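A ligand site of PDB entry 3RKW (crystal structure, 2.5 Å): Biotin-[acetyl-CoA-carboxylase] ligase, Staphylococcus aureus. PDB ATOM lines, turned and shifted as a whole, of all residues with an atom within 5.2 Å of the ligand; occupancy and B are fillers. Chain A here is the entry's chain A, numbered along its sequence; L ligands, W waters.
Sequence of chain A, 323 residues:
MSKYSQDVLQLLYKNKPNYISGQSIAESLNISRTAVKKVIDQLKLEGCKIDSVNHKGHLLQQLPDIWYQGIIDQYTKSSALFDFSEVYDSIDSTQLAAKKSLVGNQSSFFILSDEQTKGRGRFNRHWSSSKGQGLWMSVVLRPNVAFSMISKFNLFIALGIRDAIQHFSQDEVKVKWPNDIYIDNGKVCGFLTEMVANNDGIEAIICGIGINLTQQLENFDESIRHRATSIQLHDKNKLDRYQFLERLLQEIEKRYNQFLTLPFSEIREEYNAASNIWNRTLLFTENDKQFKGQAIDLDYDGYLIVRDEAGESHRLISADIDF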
ATOM      1  N   SER A  93      11.956  23.099   7.756  1.00  0.00           N
ATOM      2  CA  SER A  93      11.426  24.433   7.496  1.00  0.00           C
ATOM      3  C   SER A  93      12.271  25.510   8.178  1.00  0.00           C
ATOM      4  O   SER A  93      12.536  25.444   9.429  1.00  0.00           O
ATOM      5  CB  SER A  93       9.981  24.578   8.002  1.00  0.00           C
ATOM      6  OG  SER A  93       9.539  25.916   7.842  1.00  0.00           O
ATOM      7  N   THR A  94      12.692  26.500   7.375  1.00  0.00           N
ATOM      8  CA  THR A  94      13.321  27.713   7.946  1.00  0.00           C
ATOM      9  C   THR A  94      12.457  28.385   9.027  1.00  0.00           C
ATOM     10  O   THR A  94      12.984  28.853  10.023  1.00  0.00           O
ATOM     11  CB  THR A  94      13.703  28.771   6.914  1.00  0.00           C
ATOM     12  OG1 THR A  94      12.539  29.172   6.181  1.00  0.00           O
ATOM     13  CG2 THR A  94      14.824  28.217   5.947  1.00  0.00           C
ATOM     14  N   GLN A  95      11.135  28.357   8.829  1.00  0.00           N
ATOM     15  CA  GLN A  95      10.197  28.973   9.744  1.00  0.00           C
ATOM     16  C   GLN A  95      10.123  28.263  11.127  1.00  0.00           C
ATOM     17  O   GLN A  95      10.065  28.898  12.190  1.00  0.00           O
ATOM     18  CB  GLN A  95       8.789  29.050   9.038  1.00  0.00           C
ATOM     19  CG  GLN A  95       7.798  30.020   9.659  1.00  0.00           C
ATOM     20  CD  GLN A  95       8.080  31.512   9.322  1.00  0.00           C
ATOM     21  OE1 GLN A  95       9.078  31.888   8.723  1.00  0.00           O
ATOM     22  NE2 GLN A  95       7.168  32.361   9.746  1.00  0.00           N
ATOM     23  N   GLN A 116      13.762  22.718   1.640  1.00  0.00           N
ATOM     24  CA  GLN A 116      12.927  22.467   2.807  1.00  0.00           C
ATOM     25  C   GLN A 116      12.168  21.223   2.505  1.00  0.00           C
ATOM     26  O   GLN A 116      11.840  20.961   1.382  1.00  0.00           O
ATOM     27  CB  GLN A 116      11.961  23.616   3.140  1.00  0.00           C
ATOM     28  CG  GLN A 116      12.613  24.933   3.498  1.00  0.00           C
ATOM     29  CD  GLN A 116      11.586  26.055   3.866  1.00  0.00           C
ATOM     30  OE1 GLN A 116      11.655  26.662   4.944  1.00  0.00           O
ATOM     31  NE2 GLN A 116      10.664  26.355   2.943  1.00  0.00           N
ATOM     32  N   LYS A 118       9.626  20.269   4.518  1.00  0.00           N
ATOM     33  CA  LYS A 118       8.283  20.437   5.065  1.00  0.00           C
ATOM     34  C   LYS A 118       7.895  21.937   5.055  1.00  0.00           C
ATOM     35  O   LYS A 118       7.488  22.514   6.061  1.00  0.00           O
ATOM     36  CB  LYS A 118       8.197  19.782   6.424  1.00  0.00           C
ATOM     37  CG  LYS A 118       6.826  19.766   6.976  1.00  0.00           C
ATOM     38  CD  LYS A 118       6.781  19.250   8.404  1.00  0.00           C
ATOM     39  CE  LYS A 118       5.358  18.736   8.740  1.00  0.00           C
ATOM     40  NZ  LYS A 118       5.326  17.651   9.812  1.00  0.00           N
ATOM     41  N   GLY A 119       8.122  22.551   3.905  1.00  0.00           N
ATOM     42  CA  GLY A 119       7.752  23.936   3.670  1.00  0.00           C
ATOM     43  C   GLY A 119       6.264  24.182   3.734  1.00  0.00           C
ATOM     44  O   GLY A 119       5.489  23.483   3.114  1.00  0.00           O
ATOM     45  N   ARG A 120       5.882  25.172   4.503  1.00  0.00           N
ATOM     46  CA  ARG A 120       4.481  25.535   4.672  1.00  0.00           C
ATOM     47  C   ARG A 120       4.168  27.003   4.249  1.00  0.00           C
ATOM     48  O   ARG A 120       4.947  27.906   4.507  1.00  0.00           O
ATOM     49  CB  ARG A 120       4.088  25.210   6.093  1.00  0.00           C
ATOM     50  CG  ARG A 120       4.135  23.669   6.297  1.00  0.00           C
ATOM     51  CD  ARG A 120       3.043  22.890   5.464  1.00  0.00           C
ATOM     52  NE  ARG A 120       3.039  21.427   5.670  1.00  0.00           N
ATOM     53  CZ  ARG A 120       3.845  20.527   5.045  1.00  0.00           C
ATOM     54  NH1 ARG A 120       4.771  20.868   4.137  1.00  0.00           N
ATOM     55  NH2 ARG A 120       3.727  19.244   5.311  1.00  0.00           N
ATOM     56  N   GLY A 121       3.091  27.234   3.503  1.00  0.00           N
ATOM     57  CA  GLY A 121       2.624  28.613   3.308  1.00  0.00           C
ATOM     58  C   GLY A 121       1.547  28.866   4.344  1.00  0.00           C
ATOM     59  O   GLY A 121       1.656  28.480   5.532  1.00  0.00           O
ATOM     60  N   ARG A 122       0.467  29.486   3.923  1.00  0.00           N
ATOM     61  CA  ARG A 122      -0.702  29.811   4.825  1.00  0.00           C
ATOM     62  C   ARG A 122      -1.678  28.624   5.000  1.00  0.00           C
ATOM     63  O   ARG A 122      -1.735  27.708   4.138  1.00  0.00           O
ATOM     64  CB  ARG A 122      -1.399  31.062   4.278  1.00  0.00           C
ATOM     65  CG  ARG A 122      -0.402  32.228   4.106  1.00  0.00           C
ATOM     66  CD  ARG A 122      -0.995  33.414   3.392  1.00  0.00           C
ATOM     67  NE  ARG A 122      -2.209  33.941   4.048  1.00  0.00           N
ATOM     68  CZ  ARG A 122      -3.193  34.593   3.415  1.00  0.00           C
ATOM     69  NH1 ARG A 122      -3.133  34.762   2.115  1.00  0.00           N
ATOM     70  NH2 ARG A 122      -4.258  35.070   4.070  1.00  0.00           N
ATOM     71  N   PHE A 123      -2.395  28.625   6.118  1.00  0.00           N
ATOM     72  CA  PHE A 123      -3.397  27.584   6.394  1.00  0.00           C
ATOM     73  C   PHE A 123      -2.805  26.203   6.240  1.00  0.00           C
ATOM     74  O   PHE A 123      -3.462  25.241   5.907  1.00  0.00           O
ATOM     75  CB  PHE A 123      -4.618  27.758   5.473  1.00  0.00           C
ATOM     76  CG  PHE A 123      -5.156  29.153   5.472  1.00  0.00           C
ATOM     77  CD1 PHE A 123      -5.944  29.625   6.520  1.00  0.00           C
ATOM     78  CD2 PHE A 123      -4.833  30.018   4.412  1.00  0.00           C
ATOM     79  CE1 PHE A 123      -6.408  30.934   6.490  1.00  0.00           C
ATOM     80  CE2 PHE A 123      -5.304  31.334   4.380  1.00  0.00           C
ATOM     81  CZ  PHE A 123      -6.075  31.805   5.401  1.00  0.00           C
ATOM     82  N   ARG A 125      -0.986  25.049   3.887  1.00  0.00           N
ATOM     83  CA  ARG A 125      -0.707  24.494   2.563  1.00  0.00           C
ATOM     84  C   ARG A 125       0.767  24.158   2.371  1.00  0.00           C
ATOM     85  O   ARG A 125       1.615  24.738   3.035  1.00  0.00           O
ATOM     86  CB  ARG A 125      -1.045  25.480   1.484  1.00  0.00           C
ATOM     87  CG  ARG A 125      -2.568  26.005   1.471  1.00  0.00           C
ATOM     88  CD  ARG A 125      -2.446  27.335   0.660  1.00  0.00           C
ATOM     89  NE  ARG A 125      -3.714  27.851   0.595  1.00  0.00           N
ATOM     90  CZ  ARG A 125      -4.091  29.067   0.871  1.00  0.00           C
ATOM     91  NH1 ARG A 125      -3.273  30.041   1.161  1.00  0.00           N
ATOM     92  NH2 ARG A 125      -5.372  29.219   0.740  1.00  0.00           N
ATOM     93  N   HIS A 126       1.077  23.279   1.408  1.00  0.00           N
ATOM     94  CA  HIS A 126       2.444  22.930   1.094  1.00  0.00           C
ATOM     95  C   HIS A 126       3.125  24.084   0.323  1.00  0.00           C
ATOM     96  O   HIS A 126       2.489  24.766  -0.434  1.00  0.00           O
ATOM     97  CB  HIS A 126       2.550  21.593   0.319  1.00  0.00           C
ATOM     98  CG  HIS A 126       2.695  21.775  -1.163  1.00  0.00           C
ATOM     99  ND1 HIS A 126       3.828  21.445  -1.867  1.00  0.00           N
ATOM    100  CD2 HIS A 126       1.805  22.267  -2.061  1.00  0.00           C
ATOM    101  CE1 HIS A 126       3.631  21.741  -3.162  1.00  0.00           C
ATOM    102  NE2 HIS A 126       2.414  22.240  -3.301  1.00  0.00           N
ATOM    103  N   TRP A 127       4.413  24.341   0.567  1.00  0.00           N
ATOM    104  CA  TRP A 127       5.207  25.254  -0.200  1.00  0.00           C
ATOM    105  C   TRP A 127       6.418  24.513  -0.756  1.00  0.00           C
ATOM    106  O   TRP A 127       7.277  23.978  -0.021  1.00  0.00           O
ATOM    107  CB  TRP A 127       5.686  26.458   0.636  1.00  0.00           C
ATOM    108  CG  TRP A 127       6.471  27.444  -0.246  1.00  0.00           C
ATOM    109  CD1 TRP A 127       7.821  27.498  -0.419  1.00  0.00           C
ATOM    110  CD2 TRP A 127       5.925  28.440  -1.118  1.00  0.00           C
ATOM    111  NE1 TRP A 127       8.160  28.491  -1.312  1.00  0.00           N
ATOM    112  CE2 TRP A 127       7.020  29.089  -1.759  1.00  0.00           C
ATOM    113  CE3 TRP A 127       4.620  28.867  -1.415  1.00  0.00           C
ATOM    114  CZ2 TRP A 127       6.857  30.131  -2.690  1.00  0.00           C
ATOM    115  CZ3 TRP A 127       4.461  29.918  -2.315  1.00  0.00           C
ATOM    116  CH2 TRP A 127       5.584  30.538  -2.962  1.00  0.00           C
ATOM    117  N   SER A 128       6.507  24.511  -2.056  1.00  0.00           N
ATOM    118  CA  SER A 128       7.470  23.658  -2.745  1.00  0.00           C
ATOM    119  C   SER A 128       8.808  24.350  -2.585  1.00  0.00           C
ATOM    120  O   SER A 128       8.912  25.539  -2.909  1.00  0.00           O
ATOM    121  CB  SER A 128       7.090  23.472  -4.240  1.00  0.00           C
ATOM    122  OG  SER A 128       7.997  22.600  -4.875  1.00  0.00           O
ATOM    123  N   TRP A 136      14.808  30.246   0.324  1.00  0.00           N
ATOM    124  CA  TRP A 136      13.894  29.827   1.378  1.00  0.00           C
ATOM    125  C   TRP A 136      14.459  30.308   2.670  1.00  0.00           C
ATOM    126  O   TRP A 136      15.389  29.715   3.214  1.00  0.00           O
ATOM    127  CB  TRP A 136      13.680  28.315   1.432  1.00  0.00           C
ATOM    128  CG  TRP A 136      13.721  27.632   0.077  1.00  0.00           C
ATOM    129  CD1 TRP A 136      14.562  26.609  -0.287  1.00  0.00           C
ATOM    130  CD2 TRP A 136      12.940  27.921  -1.091  1.00  0.00           C
ATOM    131  NE1 TRP A 136      14.346  26.248  -1.584  1.00  0.00           N
ATOM    132  CE2 TRP A 136      13.357  27.025  -2.113  1.00  0.00           C
ATOM    133  CE3 TRP A 136      11.922  28.837  -1.368  1.00  0.00           C
ATOM    134  CZ2 TRP A 136      12.800  26.999  -3.363  1.00  0.00           C
ATOM    135  CZ3 TRP A 136      11.347  28.831  -2.651  1.00  0.00           C
ATOM    136  CH2 TRP A 136      11.796  27.915  -3.637  1.00  0.00           C
ATOM    137  N   MET A 137      13.866  31.372   3.170  1.00  0.00           N
ATOM    138  CA  MET A 137      14.433  32.147   4.237  1.00  0.00           C
ATOM    139  C   MET A 137      13.386  32.437   5.315  1.00  0.00           C
ATOM    140  O   MET A 137      12.194  32.653   5.030  1.00  0.00           O
ATOM    141  CB  MET A 137      14.979  33.465   3.645  1.00  0.00           C
ATOM    142  CG  MET A 137      15.777  34.328   4.623  1.00  0.00           C
ATOM    143  SD  MET A 137      16.538  35.899   4.004  1.00  0.00           S
ATOM    144  CE  MET A 137      15.268  36.470   2.939  1.00  0.00           C
ATOM    145  N   SER A 138      13.844  32.520   6.561  1.00  0.00           N
ATOM    146  CA  SER A 138      13.008  33.112   7.589  1.00  0.00           C
ATOM    147  C   SER A 138      13.735  34.237   8.235  1.00  0.00           C
ATOM    148  O   SER A 138      14.890  34.100   8.542  1.00  0.00           O
ATOM    149  CB  SER A 138      12.535  32.047   8.601  1.00  0.00           C
ATOM    150  OG  SER A 138      11.618  31.183   7.922  1.00  0.00           O
ATOM    151  N   ASN A 179       0.128  38.671   0.514  1.00  0.00           N
ATOM    152  CA  ASN A 179       1.179  37.720   0.815  1.00  0.00           C
ATOM    153  C   ASN A 179       1.918  37.122  -0.364  1.00  0.00           C
ATOM    154  O   ASN A 179       2.591  36.145  -0.174  1.00  0.00           O
ATOM    155  CB  ASN A 179       0.565  36.544   1.564  1.00  0.00           C
ATOM    156  CG  ASN A 179       0.139  36.917   2.940  1.00  0.00           C
ATOM    157  OD1 ASN A 179      -1.040  37.024   3.236  1.00  0.00           O
ATOM    158  ND2 ASN A 179       1.117  37.102   3.797  1.00  0.00           N
ATOM    159  N   ASP A 180       1.759  37.642  -1.564  1.00  0.00           N
ATOM    160  CA  ASP A 180       2.367  37.031  -2.707  1.00  0.00           C
ATOM    161  C   ASP A 180       2.907  38.083  -3.690  1.00  0.00           C
ATOM    162  O   ASP A 180       2.495  39.239  -3.667  1.00  0.00           O
ATOM    163  CB  ASP A 180       1.411  36.109  -3.418  1.00  0.00           C
ATOM    164  CG  ASP A 180       0.822  35.067  -2.511  1.00  0.00           C
ATOM    165  OD1 ASP A 180      -0.371  35.269  -2.161  1.00  0.00           O
ATOM    166  OD2 ASP A 180       1.486  34.033  -2.189  1.00  0.00           O
ATOM    167  N   LYS A 187       3.232  33.467  -9.925  1.00  0.00           N
ATOM    168  CA  LYS A 187       3.667  33.719  -8.547  1.00  0.00           C
ATOM    169  C   LYS A 187       5.201  33.412  -8.381  1.00  0.00           C
ATOM    170  O   LYS A 187       5.611  32.313  -8.578  1.00  0.00           O
ATOM    171  CB  LYS A 187       2.841  32.879  -7.565  1.00  0.00           C
ATOM    172  CG  LYS A 187       3.102  33.184  -6.099  1.00  0.00           C
ATOM    173  CD  LYS A 187       2.616  32.070  -5.218  1.00  0.00           C
ATOM    174  CE  LYS A 187       1.175  32.327  -4.746  1.00  0.00           C
ATOM    175  NZ  LYS A 187       0.782  31.481  -3.564  1.00  0.00           N
ATOM    176  N   GLY A 190       6.067  33.692  -2.223  1.00  0.00           N
ATOM    177  CA  GLY A 190       5.088  33.789  -1.179  1.00  0.00           C
ATOM    178  C   GLY A 190       5.762  34.220   0.097  1.00  0.00           C
ATOM    179  O   GLY A 190       6.892  33.851   0.432  1.00  0.00           O
ATOM    180  N   PHE A 191       5.106  35.075   0.841  1.00  0.00           N
ATOM    181  CA  PHE A 191       5.728  35.462   2.072  1.00  0.00           C
ATOM    182  C   PHE A 191       4.688  35.504   3.152  1.00  0.00           C
ATOM    183  O   PHE A 191       3.480  35.494   2.886  1.00  0.00           O
ATOM    184  CB  PHE A 191       6.547  36.748   1.896  1.00  0.00           C
ATOM    185  CG  PHE A 191       5.741  37.891   1.623  1.00  0.00           C
ATOM    186  CD1 PHE A 191       5.454  38.250   0.305  1.00  0.00           C
ATOM    187  CD2 PHE A 191       5.193  38.604   2.678  1.00  0.00           C
ATOM    188  CE1 PHE A 191       4.629  39.343   0.013  1.00  0.00           C
ATOM    189  CE2 PHE A 191       4.390  39.732   2.386  1.00  0.00           C
ATOM    190  CZ  PHE A 191       4.120  40.090   1.040  1.00  0.00           C
ATOM    191  N   LEU A 192       5.140  35.481   4.393  1.00  0.00           N
ATOM    192  CA  LEU A 192       4.196  35.246   5.455  1.00  0.00           C
ATOM    193  C   LEU A 192       4.739  35.820   6.750  1.00  0.00           C
ATOM    194  O   LEU A 192       5.865  35.537   7.121  1.00  0.00           O
ATOM    195  CB  LEU A 192       4.016  33.714   5.524  1.00  0.00           C
ATOM    196  CG  LEU A 192       3.362  33.124   6.736  1.00  0.00           C
ATOM    197  CD1 LEU A 192       1.996  33.774   6.966  1.00  0.00           C
ATOM    198  CD2 LEU A 192       3.206  31.685   6.520  1.00  0.00           C
ATOM    199  N   GLY A 208       8.461  34.635   6.969  1.00  0.00           N
ATOM    200  CA  GLY A 208       8.819  33.580   6.029  1.00  0.00           C
ATOM    201  C   GLY A 208       8.764  34.003   4.544  1.00  0.00           C
ATOM    202  O   GLY A 208       7.720  34.299   4.010  1.00  0.00           O
ATOM    203  N   ILE A 209       9.914  33.964   3.869  1.00  0.00           N
ATOM    204  CA  ILE A 209      10.008  34.385   2.511  1.00  0.00           C
ATOM    205  C   ILE A 209      10.493  33.288   1.587  1.00  0.00           C
ATOM    206  O   ILE A 209      11.606  32.796   1.704  1.00  0.00           O
ATOM    207  CB  ILE A 209      10.941  35.625   2.409  1.00  0.00           C
ATOM    208  CG1 ILE A 209      10.536  36.676   3.445  1.00  0.00           C
ATOM    209  CG2 ILE A 209      10.876  36.154   0.938  1.00  0.00           C
ATOM    210  CD1 ILE A 209      11.302  37.910   3.365  1.00  0.00           C
ATOM    211  N   GLY A 210       9.632  32.951   0.649  1.00  0.00           N
ATOM    212  CA  GLY A 210       9.878  31.942  -0.366  1.00  0.00           C
ATOM    213  C   GLY A 210       9.965  32.596  -1.735  1.00  0.00           C
ATOM    214  O   GLY A 210       8.959  33.121  -2.234  1.00  0.00           O
ATOM    215  N   ASN A 212      11.183  32.025  -5.783  1.00  0.00           N
ATOM    216  CA  ASN A 212      11.667  31.196  -6.901  1.00  0.00           C
ATOM    217  C   ASN A 212      12.800  31.898  -7.631  1.00  0.00           C
ATOM    218  O   ASN A 212      12.634  32.996  -8.091  1.00  0.00           O
ATOM    219  CB  ASN A 212      10.561  30.808  -7.874  1.00  0.00           C
ATOM    220  CG  ASN A 212       9.443  30.011  -7.209  1.00  0.00           C
ATOM    221  OD1 ASN A 212       9.683  29.165  -6.338  1.00  0.00           O
ATOM    222  ND2 ASN A 212       8.211  30.300  -7.592  1.00  0.00           N
ATOM    223  N   GLN A 215      14.465  28.071 -11.191  1.00  0.00           N
ATOM    224  CA  GLN A 215      13.613  27.086 -11.877  1.00  0.00           C
ATOM    225  C   GLN A 215      13.330  27.368 -13.352  1.00  0.00           C
ATOM    226  O   GLN A 215      13.079  28.504 -13.753  1.00  0.00           O
ATOM    227  CB  GLN A 215      12.226  26.982 -11.243  1.00  0.00           C
ATOM    228  CG  GLN A 215      12.191  26.334  -9.899  1.00  0.00           C
ATOM    229  CD  GLN A 215      11.986  27.353  -8.799  1.00  0.00           C
ATOM    230  OE1 GLN A 215      12.411  28.507  -8.943  1.00  0.00           O
ATOM    231  NE2 GLN A 215      11.296  26.964  -7.711  1.00  0.00           N
ATOM    232  N   PHE A 220       8.762  23.010 -12.019  1.00  0.00           N
ATOM    233  CA  PHE A 220       7.617  23.073 -11.134  1.00  0.00           C
ATOM    234  C   PHE A 220       6.655  21.911 -11.341  1.00  0.00           C
ATOM    235  O   PHE A 220       6.418  21.487 -12.447  1.00  0.00           O
ATOM    236  CB  PHE A 220       6.818  24.350 -11.411  1.00  0.00           C
ATOM    237  CG  PHE A 220       7.506  25.604 -11.048  1.00  0.00           C
ATOM    238  CD1 PHE A 220       7.747  25.910  -9.725  1.00  0.00           C
ATOM    239  CD2 PHE A 220       7.858  26.502 -11.995  1.00  0.00           C
ATOM    240  CE1 PHE A 220       8.388  27.085  -9.383  1.00  0.00           C
ATOM    241  CE2 PHE A 220       8.462  27.685 -11.647  1.00  0.00           C
ATOM    242  CZ  PHE A 220       8.730  27.968 -10.361  1.00  0.00           C
ATOM    243  N   ILE A 224       0.970  23.359 -10.181  1.00  0.00           N
ATOM    244  CA  ILE A 224       1.218  24.799 -10.097  1.00  0.00           C
ATOM    245  C   ILE A 224       1.948  25.452 -11.293  1.00  0.00           C
ATOM    246  O   ILE A 224       2.151  26.680 -11.365  1.00  0.00           O
ATOM    247  CB  ILE A 224       2.001  25.132  -8.775  1.00  0.00           C
ATOM    248  CG1 ILE A 224       3.447  24.632  -8.841  1.00  0.00           C
ATOM    249  CG2 ILE A 224       1.239  24.565  -7.546  1.00  0.00           C
ATOM    250  CD1 ILE A 224       4.348  25.231  -7.760  1.00  0.00           C
ATOM    251  N   ARG A 227       0.766  28.605 -13.027  1.00  0.00           N
ATOM    252  CA  ARG A 227       0.660  29.782 -12.185  1.00  0.00           C
ATOM    253  C   ARG A 227       1.939  30.022 -11.357  1.00  0.00           C
ATOM    254  O   ARG A 227       1.901  30.711 -10.344  1.00  0.00           O
ATOM    255  CB  ARG A 227      -0.627  29.731 -11.310  1.00  0.00           C
ATOM    256  CG  ARG A 227      -0.897  28.478 -10.509  1.00  0.00           C
ATOM    257  CD  ARG A 227      -2.253  28.591  -9.780  1.00  0.00           C
ATOM    258  NE  ARG A 227      -2.417  27.702  -8.610  1.00  0.00           N
ATOM    259  CZ  ARG A 227      -2.553  26.375  -8.687  1.00  0.00           C
ATOM    260  NH1 ARG A 227      -2.708  25.623  -7.604  1.00  0.00           N
ATOM    261  NH2 ARG A 227      -2.511  25.792  -9.865  1.00  0.00           N
ATOM    262  N   ALA A 228       3.079  29.484 -11.799  1.00  0.00           N
ATOM    263  CA  ALA A 228       4.348  29.713 -11.062  1.00  0.00           C
ATOM    264  C   ALA A 228       5.443  30.224 -11.959  1.00  0.00           C
ATOM    265  O   ALA A 228       5.535  29.813 -13.079  1.00  0.00           O
ATOM    266  CB  ALA A 228       4.824  28.433 -10.387  1.00  0.00           C
HETATM  267  C1  LIG L   1       2.328  31.710   1.475  1.00  0.00           C
HETATM  268  O1  LIG L   1       1.867  30.609   0.737  1.00  0.00           O
HETATM  269  C2  LIG L   1       3.712  31.999   1.497  1.00  0.00           C
HETATM  270  C3  LIG L   1       4.538  30.964   1.968  1.00  0.00           C
HETATM  271  C4  LIG L   1       5.896  31.158   2.545  1.00  0.00           C
HETATM  272  C5  LIG L   1       7.032  30.173   2.092  1.00  0.00           C
HETATM  273  C6  LIG L   1       8.346  30.438   2.671  1.00  0.00           C
HETATM  274  S1  LIG L   1       9.603  29.442   2.283  1.00  0.00           S
HETATM  275  C7  LIG L   1      10.546  29.972   3.564  1.00  0.00           C
HETATM  276  C8  LIG L   1       9.602  29.894   4.811  1.00  0.00           C
HETATM  277  N1  LIG L   1       9.533  28.663   5.463  1.00  0.00           N
HETATM  278  C9  LIG L   1       8.394  27.944   4.863  1.00  0.00           C
HETATM  279  O2  LIG L   1       8.004  26.905   5.510  1.00  0.00           O
HETATM  280  N2  LIG L   1       7.366  29.034   4.669  1.00  0.00           N
HETATM  281  C10 LIG L   1       8.128  30.140   4.242  1.00  0.00           C
HETATM  282  P1  LIG L   1       0.419  30.249   0.399  1.00  0.00           P
HETATM  283  O3  LIG L   1      -0.105  31.333  -0.414  1.00  0.00           O
HETATM  284  O4  LIG L   1      -0.291  29.887   1.604  1.00  0.00           O
HETATM  285  O5  LIG L   1       0.576  28.952  -0.453  1.00  0.00           O
HETATM  286  C11 LIG L   1       1.324  28.921  -1.596  1.00  0.00           C
HETATM  287  C12 LIG L   1       0.603  28.201  -2.693  1.00  0.00           C
HETATM  288  O6  LIG L   1       1.124  28.574  -3.990  1.00  0.00           O
HETATM  289  C13 LIG L   1       0.446  26.679  -2.703  1.00  0.00           C
HETATM  290  O7  LIG L   1      -0.740  26.234  -2.081  1.00  0.00           O
HETATM  291  C14 LIG L   1       0.458  26.372  -4.199  1.00  0.00           C
HETATM  292  O8  LIG L   1      -0.825  26.667  -4.759  1.00  0.00           O
HETATM  293  C15 LIG L   1       1.409  27.423  -4.713  1.00  0.00           C
HETATM  294  N3  LIG L   1       2.815  27.084  -4.489  1.00  0.00           N
HETATM  295  C16 LIG L   1       3.424  26.213  -3.677  1.00  0.00           C
HETATM  296  N4  LIG L   1       4.753  26.359  -3.856  1.00  0.00           N
HETATM  297  C17 LIG L   1       4.989  27.354  -4.720  1.00  0.00           C
HETATM  298  C18 LIG L   1       6.086  27.970  -5.319  1.00  0.00           C
HETATM  299  N5  LIG L   1       7.443  27.609  -5.100  1.00  0.00           N
HETATM  300  N6  LIG L   1       5.850  28.914  -6.224  1.00  0.00           N
HETATM  301  C19 LIG L   1       4.618  29.283  -6.550  1.00  0.00           C
HETATM  302  N7  LIG L   1       3.572  28.721  -6.018  1.00  0.00           N
HETATM  303  C20 LIG L   1       3.729  27.784  -5.113  1.00  0.00           C
HETATM  304  O   HOH W   1      -0.742  23.772  -1.730  1.00  0.00           O
HETATM  305  O   HOH W   2       1.361  29.302  -7.834  1.00  0.00           O
HETATM  306  O   HOH W   3      -1.258  33.672   0.279  1.00  0.00           O
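The backbone NH (N) of Ser 128 lies within hydrogen-bond range of a nitrogen (N4) of the ligand (3.1 Å). The backbone NH (N) of Arg 120 sits at hydrogen-bond distance from an oxygen (O2) of the ligand (2.9 Å). The backbone carbonyl oxygen of Arg 120 sits at hydrogen-bond distance from a nitrogen (N2) of the ligand (2.7 Å). The side-chain hydroxyl (OG1) of Thr 94 is in hydrogen-bond range of a nitrogen (N1) of the ligand (3.1 Å). The guanidinium group (NH1) of Arg 125 is in salt-bridge range of an oxygen (O4) of the ligand, 3.0 Å away. NZ of Lys 187 lies within salt-bridge range of O3 of the ligand, 3.3 Å away. O4 of the ligand sits at hydrogen-bond distance from N of Arg 122, 2.5 Å away. OG of Ser 93 is in hydrogen-bond range of O2 of the ligand, at 3.0 Å. O of Ser 128 is in hydrogen-bond range of N5 of the ligand (3.4 Å). The side-chain amide oxygen (OD1) of Asn 212 is in hydrogen-bond range of a nitrogen (N5) of the ligand (3.0 Å). The side-chain amide oxygen (OE1) of Gln 116 sits at hydrogen-bond distance from a nitrogen (N1) of the ligand, at 3.0 Å.
Gln 95 touches the ligand (CB to N1, 3.7 Å). Gly 119 touches the ligand. CA of Gly 121 touches C3 of the ligand (3.3 Å). O of His 126 touches C13 of the ligand, 3.6 Å away. CE3 of Trp 127 touches C11 of the ligand, 3.3 Å away. Met 137 touches the ligand (O to C7, 3.5 Å). Ser 138 touches the ligand (OG to C8, 3.9 Å). Asp 180 touches the ligand. Gly 190 touches the ligand. Phe 191 touches the ligand (N to C2, 3.4 Å). Gly 208 touches the ligand (O to C4, 3.9 Å). Ile 209 touches the ligand. N of Gly 210 touches C6 of the ligand (3.5 Å). Ile 224 touches the ligand. Arg 227 touches the ligand. Ala 228 touches the ligand.
The backbone NH of Thr 94 lies within hydrogen-bond range of the side-chain amide oxygen of Gln 116 (2.6 Å). The backbone NH (N) of Gly 208 lies within hydrogen-bond range of the backbone carbonyl oxygen (O) of Leu 192 (2.8 Å). The guanidinium group (NH1) of Arg 122 lies close to the side-chain amide oxygen (OD1) of Asn 179 (3.3 Å). The side-chain amide oxygen of Gln 95 lies close to the backbone NH of Gly 208 (3.3 Å). The side-chain amino group (NZ) of Lys 187 lies within salt-bridge range of the side-chain carboxylate (OD2) of Asp 180 (3.0 Å). OG of Ser 138 sits at hydrogen-bond distance from OG1 of Thr 94, at 2.8 Å. The side-chain amide oxygen (OD1) of Asn 212 lies within hydrogen-bond range of the side-chain amide nitrogen (NE2) of Gln 215 (3.1 Å). The backbone NH of Phe 191 lies within hydrogen-bond range of the backbone carbonyl oxygen of Asn 179 (2.9 Å).
Water W3 lies within hydrogen-bond range of O3 of the ligand, NH1 of Arg 122 and OD1 of Asp 180. Water W2 lies within hydrogen-bond range of N7 of the ligand (2.9 Å) and O of Arg 227 (2.9 Å).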
